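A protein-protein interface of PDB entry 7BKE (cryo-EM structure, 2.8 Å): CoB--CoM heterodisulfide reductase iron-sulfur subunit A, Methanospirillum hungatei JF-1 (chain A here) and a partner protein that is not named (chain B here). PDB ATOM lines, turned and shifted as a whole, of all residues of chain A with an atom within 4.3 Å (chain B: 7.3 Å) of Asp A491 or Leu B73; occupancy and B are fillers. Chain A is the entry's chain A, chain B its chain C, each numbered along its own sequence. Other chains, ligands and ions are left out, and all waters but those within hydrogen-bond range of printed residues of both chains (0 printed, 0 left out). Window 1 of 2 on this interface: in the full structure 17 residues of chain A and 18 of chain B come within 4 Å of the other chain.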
ATOM      1  N   ILE A 469      -5.779 -22.462 -11.062  1.00  0.00           N
ATOM      2  CA  ILE A 469      -5.462 -23.465 -12.066  1.00  0.00           C
ATOM      3  C   ILE A 469      -4.524 -24.463 -11.417  1.00  0.00           C
ATOM      4  O   ILE A 469      -3.386 -24.124 -11.085  1.00  0.00           O
ATOM      5  CB  ILE A 469      -4.834 -22.834 -13.313  1.00  0.00           C
ATOM      6  CG1 ILE A 469      -5.842 -21.916 -13.993  1.00  0.00           C
ATOM      7  CG2 ILE A 469      -4.358 -23.894 -14.266  1.00  0.00           C
ATOM      8  CD1 ILE A 469      -5.221 -20.839 -14.819  1.00  0.00           C
ATOM      9  N   ARG A 470      -4.984 -25.694 -11.228  1.00  0.00           N
ATOM     10  CA  ARG A 470      -4.151 -26.703 -10.583  1.00  0.00           C
ATOM     11  C   ARG A 470      -3.195 -27.278 -11.609  1.00  0.00           C
ATOM     12  O   ARG A 470      -3.478 -28.276 -12.267  1.00  0.00           O
ATOM     13  CB  ARG A 470      -4.982 -27.800  -9.948  1.00  0.00           C
ATOM     14  CG  ARG A 470      -4.152 -28.655  -9.035  1.00  0.00           C
ATOM     15  CD  ARG A 470      -4.789 -29.970  -8.754  1.00  0.00           C
ATOM     16  NE  ARG A 470      -3.884 -30.868  -8.056  1.00  0.00           N
ATOM     17  CZ  ARG A 470      -2.925 -31.573  -8.643  1.00  0.00           C
ATOM     18  NH1 ARG A 470      -2.737 -31.487  -9.947  1.00  0.00           N
ATOM     19  NH2 ARG A 470      -2.155 -32.363  -7.922  1.00  0.00           N
ATOM     20  N   THR A 489       1.396 -24.585 -18.856  1.00  0.00           N
ATOM     21  CA  THR A 489       1.259 -25.712 -17.955  1.00  0.00           C
ATOM     22  C   THR A 489       0.050 -26.509 -18.411  1.00  0.00           C
ATOM     23  O   THR A 489      -0.476 -26.291 -19.505  1.00  0.00           O
ATOM     24  CB  THR A 489       1.148 -25.258 -16.495  1.00  0.00           C
ATOM     25  OG1 THR A 489       1.051 -26.407 -15.646  1.00  0.00           O
ATOM     26  CG2 THR A 489      -0.055 -24.370 -16.277  1.00  0.00           C
ATOM     27  N   GLU A 490      -0.374 -27.456 -17.595  1.00  0.00           N
ATOM     28  CA  GLU A 490      -1.613 -28.168 -17.825  1.00  0.00           C
ATOM     29  C   GLU A 490      -2.575 -27.850 -16.697  1.00  0.00           C
ATOM     30  O   GLU A 490      -2.179 -27.803 -15.530  1.00  0.00           O
ATOM     31  CB  GLU A 490      -1.392 -29.675 -17.908  1.00  0.00           C
ATOM     32  CG  GLU A 490      -2.632 -30.443 -18.309  1.00  0.00           C
ATOM     33  CD  GLU A 490      -2.643 -31.860 -17.786  1.00  0.00           C
ATOM     34  OE1 GLU A 490      -1.733 -32.209 -17.016  1.00  0.00           O
ATOM     35  OE2 GLU A 490      -3.556 -32.628 -18.145  1.00  0.00           O
ATOM     36  N   ASP A 491      -3.832 -27.604 -17.044  1.00  0.00           N
ATOM     37  CA  ASP A 491      -4.898 -27.577 -16.053  1.00  0.00           C
ATOM     38  C   ASP A 491      -5.249 -29.023 -15.758  1.00  0.00           C
ATOM     39  O   ASP A 491      -5.986 -29.660 -16.508  1.00  0.00           O
ATOM     40  CB  ASP A 491      -6.100 -26.793 -16.557  1.00  0.00           C
ATOM     41  CG  ASP A 491      -7.034 -26.375 -15.438  1.00  0.00           C
ATOM     42  OD1 ASP A 491      -6.942 -26.933 -14.323  1.00  0.00           O
ATOM     43  OD2 ASP A 491      -7.870 -25.485 -15.674  1.00  0.00           O
ATOM     44  N   THR A 492      -4.707 -29.541 -14.663  1.00  0.00           N
ATOM     45  CA  THR A 492      -4.837 -30.956 -14.352  1.00  0.00           C
ATOM     46  C   THR A 492      -6.281 -31.352 -14.086  1.00  0.00           C
ATOM     47  O   THR A 492      -6.688 -32.467 -14.427  1.00  0.00           O
ATOM     48  CB  THR A 492      -3.946 -31.288 -13.160  1.00  0.00           C
ATOM     49  OG1 THR A 492      -2.596 -30.925 -13.464  1.00  0.00           O
ATOM     50  CG2 THR A 492      -3.974 -32.741 -12.879  1.00  0.00           C
ATOM     51  N   LEU A 493      -7.073 -30.467 -13.480  1.00  0.00           N
ATOM     52  CA  LEU A 493      -8.480 -30.775 -13.246  1.00  0.00           C
ATOM     53  C   LEU A 493      -9.293 -30.677 -14.528  1.00  0.00           C
ATOM     54  O   LEU A 493     -10.138 -31.534 -14.801  1.00  0.00           O
ATOM     55  CB  LEU A 493      -9.046 -29.845 -12.180  1.00  0.00           C
ATOM     56  CG  LEU A 493      -8.229 -29.794 -10.897  1.00  0.00           C
ATOM     57  CD1 LEU A 493      -8.722 -28.700  -9.982  1.00  0.00           C
ATOM     58  CD2 LEU A 493      -8.267 -31.121 -10.210  1.00  0.00           C
ATOM     59  N   LEU A 494      -9.055 -29.641 -15.330  1.00  0.00           N
ATOM     60  CA  LEU A 494      -9.708 -29.548 -16.629  1.00  0.00           C
ATOM     61  C   LEU A 494      -9.234 -30.643 -17.573  1.00  0.00           C
ATOM     62  O   LEU A 494     -10.023 -31.148 -18.376  1.00  0.00           O
ATOM     63  CB  LEU A 494      -9.454 -28.177 -17.237  1.00  0.00           C
ATOM     64  CG  LEU A 494     -10.199 -27.865 -18.522  1.00  0.00           C
ATOM     65  CD1 LEU A 494     -11.681 -27.791 -18.249  1.00  0.00           C
ATOM     66  CD2 LEU A 494      -9.694 -26.563 -19.104  1.00  0.00           C
ATOM     67  N   GLY A 495      -7.966 -31.027 -17.484  1.00  0.00           N
ATOM     68  CA  GLY A 495      -7.418 -32.064 -18.330  1.00  0.00           C
ATOM     69  C   GLY A 495      -6.885 -31.599 -19.660  1.00  0.00           C
ATOM     70  O   GLY A 495      -6.791 -32.405 -20.587  1.00  0.00           O
ATOM     71  N   ARG A 496      -6.550 -30.325 -19.797  1.00  0.00           N
ATOM     72  CA  ARG A 496      -6.031 -29.788 -21.039  1.00  0.00           C
ATOM     73  C   ARG A 496      -4.808 -28.934 -20.753  1.00  0.00           C
ATOM     74  O   ARG A 496      -4.702 -28.337 -19.680  1.00  0.00           O
ATOM     75  CB  ARG A 496      -7.083 -28.936 -21.763  1.00  0.00           C
ATOM     76  CG  ARG A 496      -8.377 -29.664 -22.074  1.00  0.00           C
ATOM     77  CD  ARG A 496      -9.500 -28.698 -22.420  1.00  0.00           C
ATOM     78  NE  ARG A 496      -9.093 -27.722 -23.421  1.00  0.00           N
ATOM     79  CZ  ARG A 496      -9.771 -26.616 -23.707  1.00  0.00           C
ATOM     80  NH1 ARG A 496     -10.896 -26.340 -23.068  1.00  0.00           N
ATOM     81  NH2 ARG A 496      -9.322 -25.786 -24.630  1.00  0.00           N
ATOM     82  N   VAL A 498      -2.676 -25.477 -21.129  1.00  0.00           N
ATOM     83  CA  VAL A 498      -3.118 -24.091 -21.115  1.00  0.00           C
ATOM     84  C   VAL A 498      -1.968 -23.205 -21.570  1.00  0.00           C
ATOM     85  O   VAL A 498      -0.800 -23.579 -21.494  1.00  0.00           O
ATOM     86  CB  VAL A 498      -3.616 -23.635 -19.725  1.00  0.00           C
ATOM     87  CG1 VAL A 498      -4.760 -24.491 -19.249  1.00  0.00           C
ATOM     88  CG2 VAL A 498      -2.500 -23.647 -18.729  1.00  0.00           C
ATOM     89  N   TYR B  20      -6.086 -24.380 -23.671  1.00  0.00           N
ATOM     90  CA  TYR B  20      -6.946 -23.311 -23.183  1.00  0.00           C
ATOM     91  C   TYR B  20      -6.218 -21.974 -23.222  1.00  0.00           C
ATOM     92  O   TYR B  20      -5.103 -21.846 -22.717  1.00  0.00           O
ATOM     93  CB  TYR B  20      -7.409 -23.622 -21.758  1.00  0.00           C
ATOM     94  CG  TYR B  20      -8.060 -22.451 -21.053  1.00  0.00           C
ATOM     95  CD1 TYR B  20      -9.397 -22.155 -21.249  1.00  0.00           C
ATOM     96  CD2 TYR B  20      -7.332 -21.640 -20.194  1.00  0.00           C
ATOM     97  CE1 TYR B  20      -9.989 -21.090 -20.616  1.00  0.00           C
ATOM     98  CE2 TYR B  20      -7.918 -20.571 -19.559  1.00  0.00           C
ATOM     99  CZ  TYR B  20      -9.246 -20.301 -19.773  1.00  0.00           C
ATOM    100  OH  TYR B  20      -9.833 -19.236 -19.137  1.00  0.00           O
ATOM    101  N   HIS B  21      -6.858 -20.977 -23.819  1.00  0.00           N
ATOM    102  CA  HIS B  21      -6.364 -19.612 -23.852  1.00  0.00           C
ATOM    103  C   HIS B  21      -7.307 -18.719 -23.064  1.00  0.00           C
ATOM    104  O   HIS B  21      -8.464 -19.068 -22.823  1.00  0.00           O
ATOM    105  CB  HIS B  21      -6.251 -19.092 -25.287  1.00  0.00           C
ATOM    106  CG  HIS B  21      -5.164 -19.738 -26.078  1.00  0.00           C
ATOM    107  ND1 HIS B  21      -5.407 -20.742 -26.987  1.00  0.00           N
ATOM    108  CD2 HIS B  21      -3.828 -19.529 -26.093  1.00  0.00           C
ATOM    109  CE1 HIS B  21      -4.265 -21.125 -27.530  1.00  0.00           C
ATOM    110  NE2 HIS B  21      -3.292 -20.404 -27.005  1.00  0.00           N
ATOM    111  N   LEU B  22      -6.808 -17.548 -22.664  1.00  0.00           N
ATOM    112  CA  LEU B  22      -7.671 -16.576 -22.005  1.00  0.00           C
ATOM    113  C   LEU B  22      -8.676 -15.944 -22.953  1.00  0.00           C
ATOM    114  O   LEU B  22      -9.587 -15.251 -22.492  1.00  0.00           O
ATOM    115  CB  LEU B  22      -6.844 -15.475 -21.346  1.00  0.00           C
ATOM    116  CG  LEU B  22      -6.031 -15.883 -20.124  1.00  0.00           C
ATOM    117  CD1 LEU B  22      -5.593 -14.655 -19.366  1.00  0.00           C
ATOM    118  CD2 LEU B  22      -6.823 -16.812 -19.235  1.00  0.00           C
ATOM    119  N   ASP B  24     -10.660 -17.784 -24.539  1.00  0.00           N
ATOM    120  CA  ASP B  24     -11.725 -18.774 -24.497  1.00  0.00           C
ATOM    121  C   ASP B  24     -12.744 -18.510 -23.402  1.00  0.00           C
ATOM    122  O   ASP B  24     -13.790 -19.163 -23.381  1.00  0.00           O
ATOM    123  CB  ASP B  24     -11.132 -20.171 -24.292  1.00  0.00           C
ATOM    124  CG  ASP B  24     -10.145 -20.549 -25.371  1.00  0.00           C
ATOM    125  OD1 ASP B  24      -9.503 -21.611 -25.247  1.00  0.00           O
ATOM    126  OD2 ASP B  24     -10.020 -19.785 -26.350  1.00  0.00           O
ATOM    127  N   THR B  25     -12.466 -17.582 -22.493  1.00  0.00           N
ATOM    128  CA  THR B  25     -13.334 -17.348 -21.352  1.00  0.00           C
ATOM    129  C   THR B  25     -14.457 -16.391 -21.730  1.00  0.00           C
ATOM    130  O   THR B  25     -14.219 -15.371 -22.379  1.00  0.00           O
ATOM    131  CB  THR B  25     -12.522 -16.788 -20.190  1.00  0.00           C
ATOM    132  OG1 THR B  25     -11.647 -17.805 -19.689  1.00  0.00           O
ATOM    133  CG2 THR B  25     -13.429 -16.318 -19.076  1.00  0.00           C
ATOM    134  N   ASN B  26     -15.684 -16.725 -21.320  1.00  0.00           N
ATOM    135  CA  ASN B  26     -16.859 -15.878 -21.518  1.00  0.00           C
ATOM    136  C   ASN B  26     -17.436 -15.512 -20.154  1.00  0.00           C
ATOM    137  O   ASN B  26     -18.294 -16.229 -19.603  1.00  0.00           O
ATOM    138  CB  ASN B  26     -17.898 -16.571 -22.391  1.00  0.00           C
ATOM    139  CG  ASN B  26     -18.671 -15.597 -23.254  1.00  0.00           C
ATOM    140  OD1 ASN B  26     -18.557 -14.383 -23.095  1.00  0.00           O
ATOM    141  ND2 ASN B  26     -19.456 -16.125 -24.181  1.00  0.00           N
ATOM    142  N   PRO B  27     -16.980 -14.407 -19.566  1.00  0.00           N
ATOM    143  CA  PRO B  27     -17.547 -13.975 -18.281  1.00  0.00           C
ATOM    144  C   PRO B  27     -19.028 -13.675 -18.358  1.00  0.00           C
ATOM    145  O   PRO B  27     -19.736 -13.852 -17.362  1.00  0.00           O
ATOM    146  CB  PRO B  27     -16.727 -12.725 -17.938  1.00  0.00           C
ATOM    147  CG  PRO B  27     -16.172 -12.265 -19.232  1.00  0.00           C
ATOM    148  CD  PRO B  27     -15.943 -13.485 -20.055  1.00  0.00           C
ATOM    149  N   PHE B  29     -21.135 -15.425 -20.141  1.00  0.00           N
ATOM    150  CA  PHE B  29     -21.708 -16.755 -19.984  1.00  0.00           C
ATOM    151  C   PHE B  29     -21.738 -17.163 -18.520  1.00  0.00           C
ATOM    152  O   PHE B  29     -22.750 -17.678 -18.028  1.00  0.00           O
ATOM    153  CB  PHE B  29     -20.904 -17.755 -20.813  1.00  0.00           C
ATOM    154  CG  PHE B  29     -21.185 -19.194 -20.506  1.00  0.00           C
ATOM    155  CD1 PHE B  29     -22.337 -19.804 -20.958  1.00  0.00           C
ATOM    156  CD2 PHE B  29     -20.270 -19.952 -19.804  1.00  0.00           C
ATOM    157  CE1 PHE B  29     -22.579 -21.132 -20.696  1.00  0.00           C
ATOM    158  CE2 PHE B  29     -20.509 -21.281 -19.540  1.00  0.00           C
ATOM    159  CZ  PHE B  29     -21.662 -21.871 -19.984  1.00  0.00           C
ATOM    160  N   THR B  30     -20.643 -16.914 -17.797  1.00  0.00           N
ATOM    161  CA  THR B  30     -20.622 -17.263 -16.380  1.00  0.00           C
ATOM    162  C   THR B  30     -21.681 -16.491 -15.599  1.00  0.00           C
ATOM    163  O   THR B  30     -22.353 -17.054 -14.726  1.00  0.00           O
ATOM    164  CB  THR B  30     -19.239 -17.004 -15.790  1.00  0.00           C
ATOM    165  OG1 THR B  30     -18.240 -17.578 -16.638  1.00  0.00           O
ATOM    166  CG2 THR B  30     -19.133 -17.623 -14.413  1.00  0.00           C
ATOM    167  N   GLN B  46     -13.538 -28.267  -6.989  1.00  0.00           N
ATOM    168  CA  GLN B  46     -13.210 -29.464  -7.763  1.00  0.00           C
ATOM    169  C   GLN B  46     -12.829 -30.645  -6.879  1.00  0.00           C
ATOM    170  O   GLN B  46     -11.835 -31.325  -7.112  1.00  0.00           O
ATOM    171  CB  GLN B  46     -12.106 -29.161  -8.771  1.00  0.00           C
ATOM    172  CG  GLN B  46     -12.459 -28.063  -9.739  1.00  0.00           C
ATOM    173  CD  GLN B  46     -13.327 -28.558 -10.857  1.00  0.00           C
ATOM    174  OE1 GLN B  46     -13.004 -29.539 -11.511  1.00  0.00           O
ATOM    175  NE2 GLN B  46     -14.437 -27.885 -11.087  1.00  0.00           N
ATOM    176  N   PHE B  67     -18.333 -30.098 -16.062  1.00  0.00           N
ATOM    177  CA  PHE B  67     -19.251 -29.020 -16.425  1.00  0.00           C
ATOM    178  C   PHE B  67     -19.134 -27.834 -15.471  1.00  0.00           C
ATOM    179  O   PHE B  67     -19.225 -26.676 -15.894  1.00  0.00           O
ATOM    180  CB  PHE B  67     -20.681 -29.542 -16.472  1.00  0.00           C
ATOM    181  CG  PHE B  67     -21.063 -30.100 -17.798  1.00  0.00           C
ATOM    182  CD1 PHE B  67     -21.303 -29.262 -18.867  1.00  0.00           C
ATOM    183  CD2 PHE B  67     -21.157 -31.458 -17.986  1.00  0.00           C
ATOM    184  CE1 PHE B  67     -21.641 -29.770 -20.090  1.00  0.00           C
ATOM    185  CE2 PHE B  67     -21.495 -31.970 -19.204  1.00  0.00           C
ATOM    186  CZ  PHE B  67     -21.739 -31.125 -20.259  1.00  0.00           C
ATOM    187  N   MET B  68     -18.931 -28.100 -14.181  1.00  0.00           N
ATOM    188  CA  MET B  68     -18.721 -27.017 -13.225  1.00  0.00           C
ATOM    189  C   MET B  68     -17.452 -26.239 -13.545  1.00  0.00           C
ATOM    190  O   MET B  68     -17.426 -25.006 -13.453  1.00  0.00           O
ATOM    191  CB  MET B  68     -18.652 -27.570 -11.802  1.00  0.00           C
ATOM    192  CG  MET B  68     -19.924 -28.234 -11.322  1.00  0.00           C
ATOM    193  SD  MET B  68     -21.337 -27.129 -11.224  1.00  0.00           S
ATOM    194  CE  MET B  68     -20.618 -25.705 -10.425  1.00  0.00           C
ATOM    195  N   ARG B  69     -16.385 -26.947 -13.909  1.00  0.00           N
ATOM    196  CA  ARG B  69     -15.144 -26.284 -14.285  1.00  0.00           C
ATOM    197  C   ARG B  69     -15.329 -25.426 -15.528  1.00  0.00           C
ATOM    198  O   ARG B  69     -14.804 -24.310 -15.604  1.00  0.00           O
ATOM    199  CB  ARG B  69     -14.050 -27.321 -14.508  1.00  0.00           C
ATOM    200  CG  ARG B  69     -12.680 -26.733 -14.670  1.00  0.00           C
ATOM    201  CD  ARG B  69     -12.087 -26.375 -13.333  1.00  0.00           C
ATOM    202  NE  ARG B  69     -10.859 -25.612 -13.477  1.00  0.00           N
ATOM    203  CZ  ARG B  69     -10.622 -24.454 -12.878  1.00  0.00           C
ATOM    204  NH1 ARG B  69     -11.534 -23.920 -12.082  1.00  0.00           N
ATOM    205  NH2 ARG B  69      -9.470 -23.834 -13.072  1.00  0.00           N
ATOM    206  N   ARG B  70     -16.066 -25.934 -16.516  1.00  0.00           N
ATOM    207  CA  ARG B  70     -16.346 -25.146 -17.710  1.00  0.00           C
ATOM    208  C   ARG B  70     -17.147 -23.901 -17.368  1.00  0.00           C
ATOM    209  O   ARG B  70     -16.897 -22.828 -17.916  1.00  0.00           O
ATOM    210  CB  ARG B  70     -17.101 -25.979 -18.733  1.00  0.00           C
ATOM    211  CG  ARG B  70     -16.275 -27.008 -19.431  1.00  0.00           C
ATOM    212  CD  ARG B  70     -17.174 -27.985 -20.117  1.00  0.00           C
ATOM    213  NE  ARG B  70     -16.431 -28.982 -20.867  1.00  0.00           N
ATOM    214  CZ  ARG B  70     -16.917 -30.169 -21.189  1.00  0.00           C
ATOM    215  NH1 ARG B  70     -18.147 -30.499 -20.832  1.00  0.00           N
ATOM    216  NH2 ARG B  70     -16.179 -31.024 -21.876  1.00  0.00           N
ATOM    217  N   CYS B  71     -18.126 -24.028 -16.472  1.00  0.00           N
ATOM    218  CA  CYS B  71     -18.868 -22.857 -16.020  1.00  0.00           C
ATOM    219  C   CYS B  71     -17.949 -21.831 -15.374  1.00  0.00           C
ATOM    220  O   CYS B  71     -18.041 -20.633 -15.657  1.00  0.00           O
ATOM    221  CB  CYS B  71     -19.958 -23.276 -15.042  1.00  0.00           C
ATOM    222  SG  CYS B  71     -20.864 -21.890 -14.369  1.00  0.00           S
ATOM    223  N   VAL B  72     -17.055 -22.287 -14.496  1.00  0.00           N
ATOM    224  CA  VAL B  72     -16.160 -21.365 -13.802  1.00  0.00           C
ATOM    225  C   VAL B  72     -15.245 -20.652 -14.790  1.00  0.00           C
ATOM    226  O   VAL B  72     -15.047 -19.436 -14.707  1.00  0.00           O
ATOM    227  CB  VAL B  72     -15.357 -22.114 -12.724  1.00  0.00           C
ATOM    228  CG1 VAL B  72     -14.135 -21.318 -12.327  1.00  0.00           C
ATOM    229  CG2 VAL B  72     -16.228 -22.382 -11.521  1.00  0.00           C
ATOM    230  N   LEU B  73     -14.690 -21.390 -15.750  1.00  0.00           N
ATOM    231  CA  LEU B  73     -13.762 -20.810 -16.712  1.00  0.00           C
ATOM    232  C   LEU B  73     -14.451 -20.117 -17.877  1.00  0.00           C
ATOM    233  O   LEU B  73     -13.762 -19.517 -18.703  1.00  0.00           O
ATOM    234  CB  LEU B  73     -12.822 -21.887 -17.251  1.00  0.00           C
ATOM    235  CG  LEU B  73     -11.889 -22.520 -16.225  1.00  0.00           C
ATOM    236  CD1 LEU B  73     -11.214 -23.731 -16.813  1.00  0.00           C
ATOM    237  CD2 LEU B  73     -10.867 -21.514 -15.756  1.00  0.00           C
ATOM    238  N   GLY B  74     -15.774 -20.185 -17.978  1.00  0.00           N
ATOM    239  CA  GLY B  74     -16.460 -19.476 -19.036  1.00  0.00           C
ATOM    240  C   GLY B  74     -16.397 -20.150 -20.383  1.00  0.00           C
ATOM    241  O   GLY B  74     -16.472 -19.473 -21.409  1.00  0.00           O
ATOM    242  N   LEU B  75     -16.267 -21.474 -20.413  1.00  0.00           N
ATOM    243  CA  LEU B  75     -16.094 -22.205 -21.668  1.00  0.00           C
ATOM    244  C   LEU B  75     -17.461 -22.473 -22.295  1.00  0.00           C
ATOM    245  O   LEU B  75     -17.999 -23.584 -22.289  1.00  0.00           O
ATOM    246  CB  LEU B  75     -15.299 -23.478 -21.431  1.00  0.00           C
ATOM    247  CG  LEU B  75     -13.890 -23.175 -20.916  1.00  0.00           C
ATOM    248  CD1 LEU B  75     -13.055 -24.419 -20.832  1.00  0.00           C
ATOM    249  CD2 LEU B  75     -13.235 -22.159 -21.816  1.00  0.00           C
ATOM    250  N   GLU B  76     -18.047 -21.385 -22.782  1.00  0.00           N
ATOM    251  CA  GLU B  76     -19.185 -21.433 -23.684  1.00  0.00           C
ATOM    252  C   GLU B  76     -18.716 -21.935 -25.043  1.00  0.00           C
ATOM    253  O   GLU B  76     -17.600 -21.641 -25.482  1.00  0.00           O
ATOM    254  CB  GLU B  76     -19.812 -20.036 -23.758  1.00  0.00           C
ATOM    255  CG  GLU B  76     -21.158 -19.875 -24.447  1.00  0.00           C
ATOM    256  CD  GLU B  76     -21.044 -19.554 -25.922  1.00  0.00           C
ATOM    257  OE1 GLU B  76     -20.036 -18.934 -26.323  1.00  0.00           O
ATOM    258  OE2 GLU B  76     -21.981 -19.881 -26.678  1.00  0.00           O
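Glu A490 touches none of the printed residues of chain B. Of chain B, only Arg B69 (3.5 Å) and Leu B73 (3.9 Å) come within 4 Å of Asp A491. Printed residues of chain B within 4 Å of Leu A493: Gln B46. Of the printed residues of chain B, Leu A494 touches Arg B69 (3.9 Å) and Leu B73 (3.9 Å). Of the printed residues of chain B, Val A498 touches Tyr B20 (3.4 Å). Of the printed residues of chain A, Gln B46 touches Leu A493 (3.6 Å). Of the printed residues of chain A, Arg B69 touches Asp A491 and Leu A494. Leu B73 touches two residues of chain A. The nearest residue of chain B that does not touch Asp A491 is Tyr B20 (6.0 Å). The nearest printed residue of chain A that does not touch Leu B73 is Ile A469 (5.3 Å).
Among the printed residues, pairs that only touch across the chains: Val A498 with Tyr B20 (3.4 Å), Leu A493 with Gln B46 (3.6 Å), Arg A496 with Leu B75 (3.7 Å), Arg A496 with Tyr B20 (3.7 Å), Leu A494 with Arg B69 (3.9 Å), Asp A491 with Leu B73 (3.9 Å) and Leu A494 with Leu B73 (3.9 Å).
Of the 11 printed residues of chain A, 5 touch a printed residue of chain B. Hydrophobic or aromatic side chains of chain A that line the printed part of chain B: Leu A493, Leu A494 and Val A498. Printed residues of chain B that touch a printed residue of chain A: Tyr B20, Gln B46, Arg B69, Leu B73 and Leu B75. Hydrophobic or aromatic side chains of chain B that line the printed part of chain A: Tyr B20, Leu B73 and Leu B75. Among the printed residues, 8 pairs touch across the chains.
The backbone NH (N) of Val A498 is in hydrogen-bond range of the backbone carbonyl oxygen (O) of Thr A489. N of Asp A491 lies within hydrogen-bond range of O of Arg A496 (2.9 Å). The side-chain hydroxyl (OG1) of Thr B25 is in hydrogen-bond range of the backbone carbonyl oxygen (O) of Leu B73 (2.9 Å). The backbone NH (N) of Leu B75 lies within hydrogen-bond range of the backbone carbonyl oxygen (O) of Arg B70 (2.9 Å).
The side-chain carboxylate of Asp A491 is in salt-bridge range of the guanidinium group of Arg B69 (3.5 Å).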
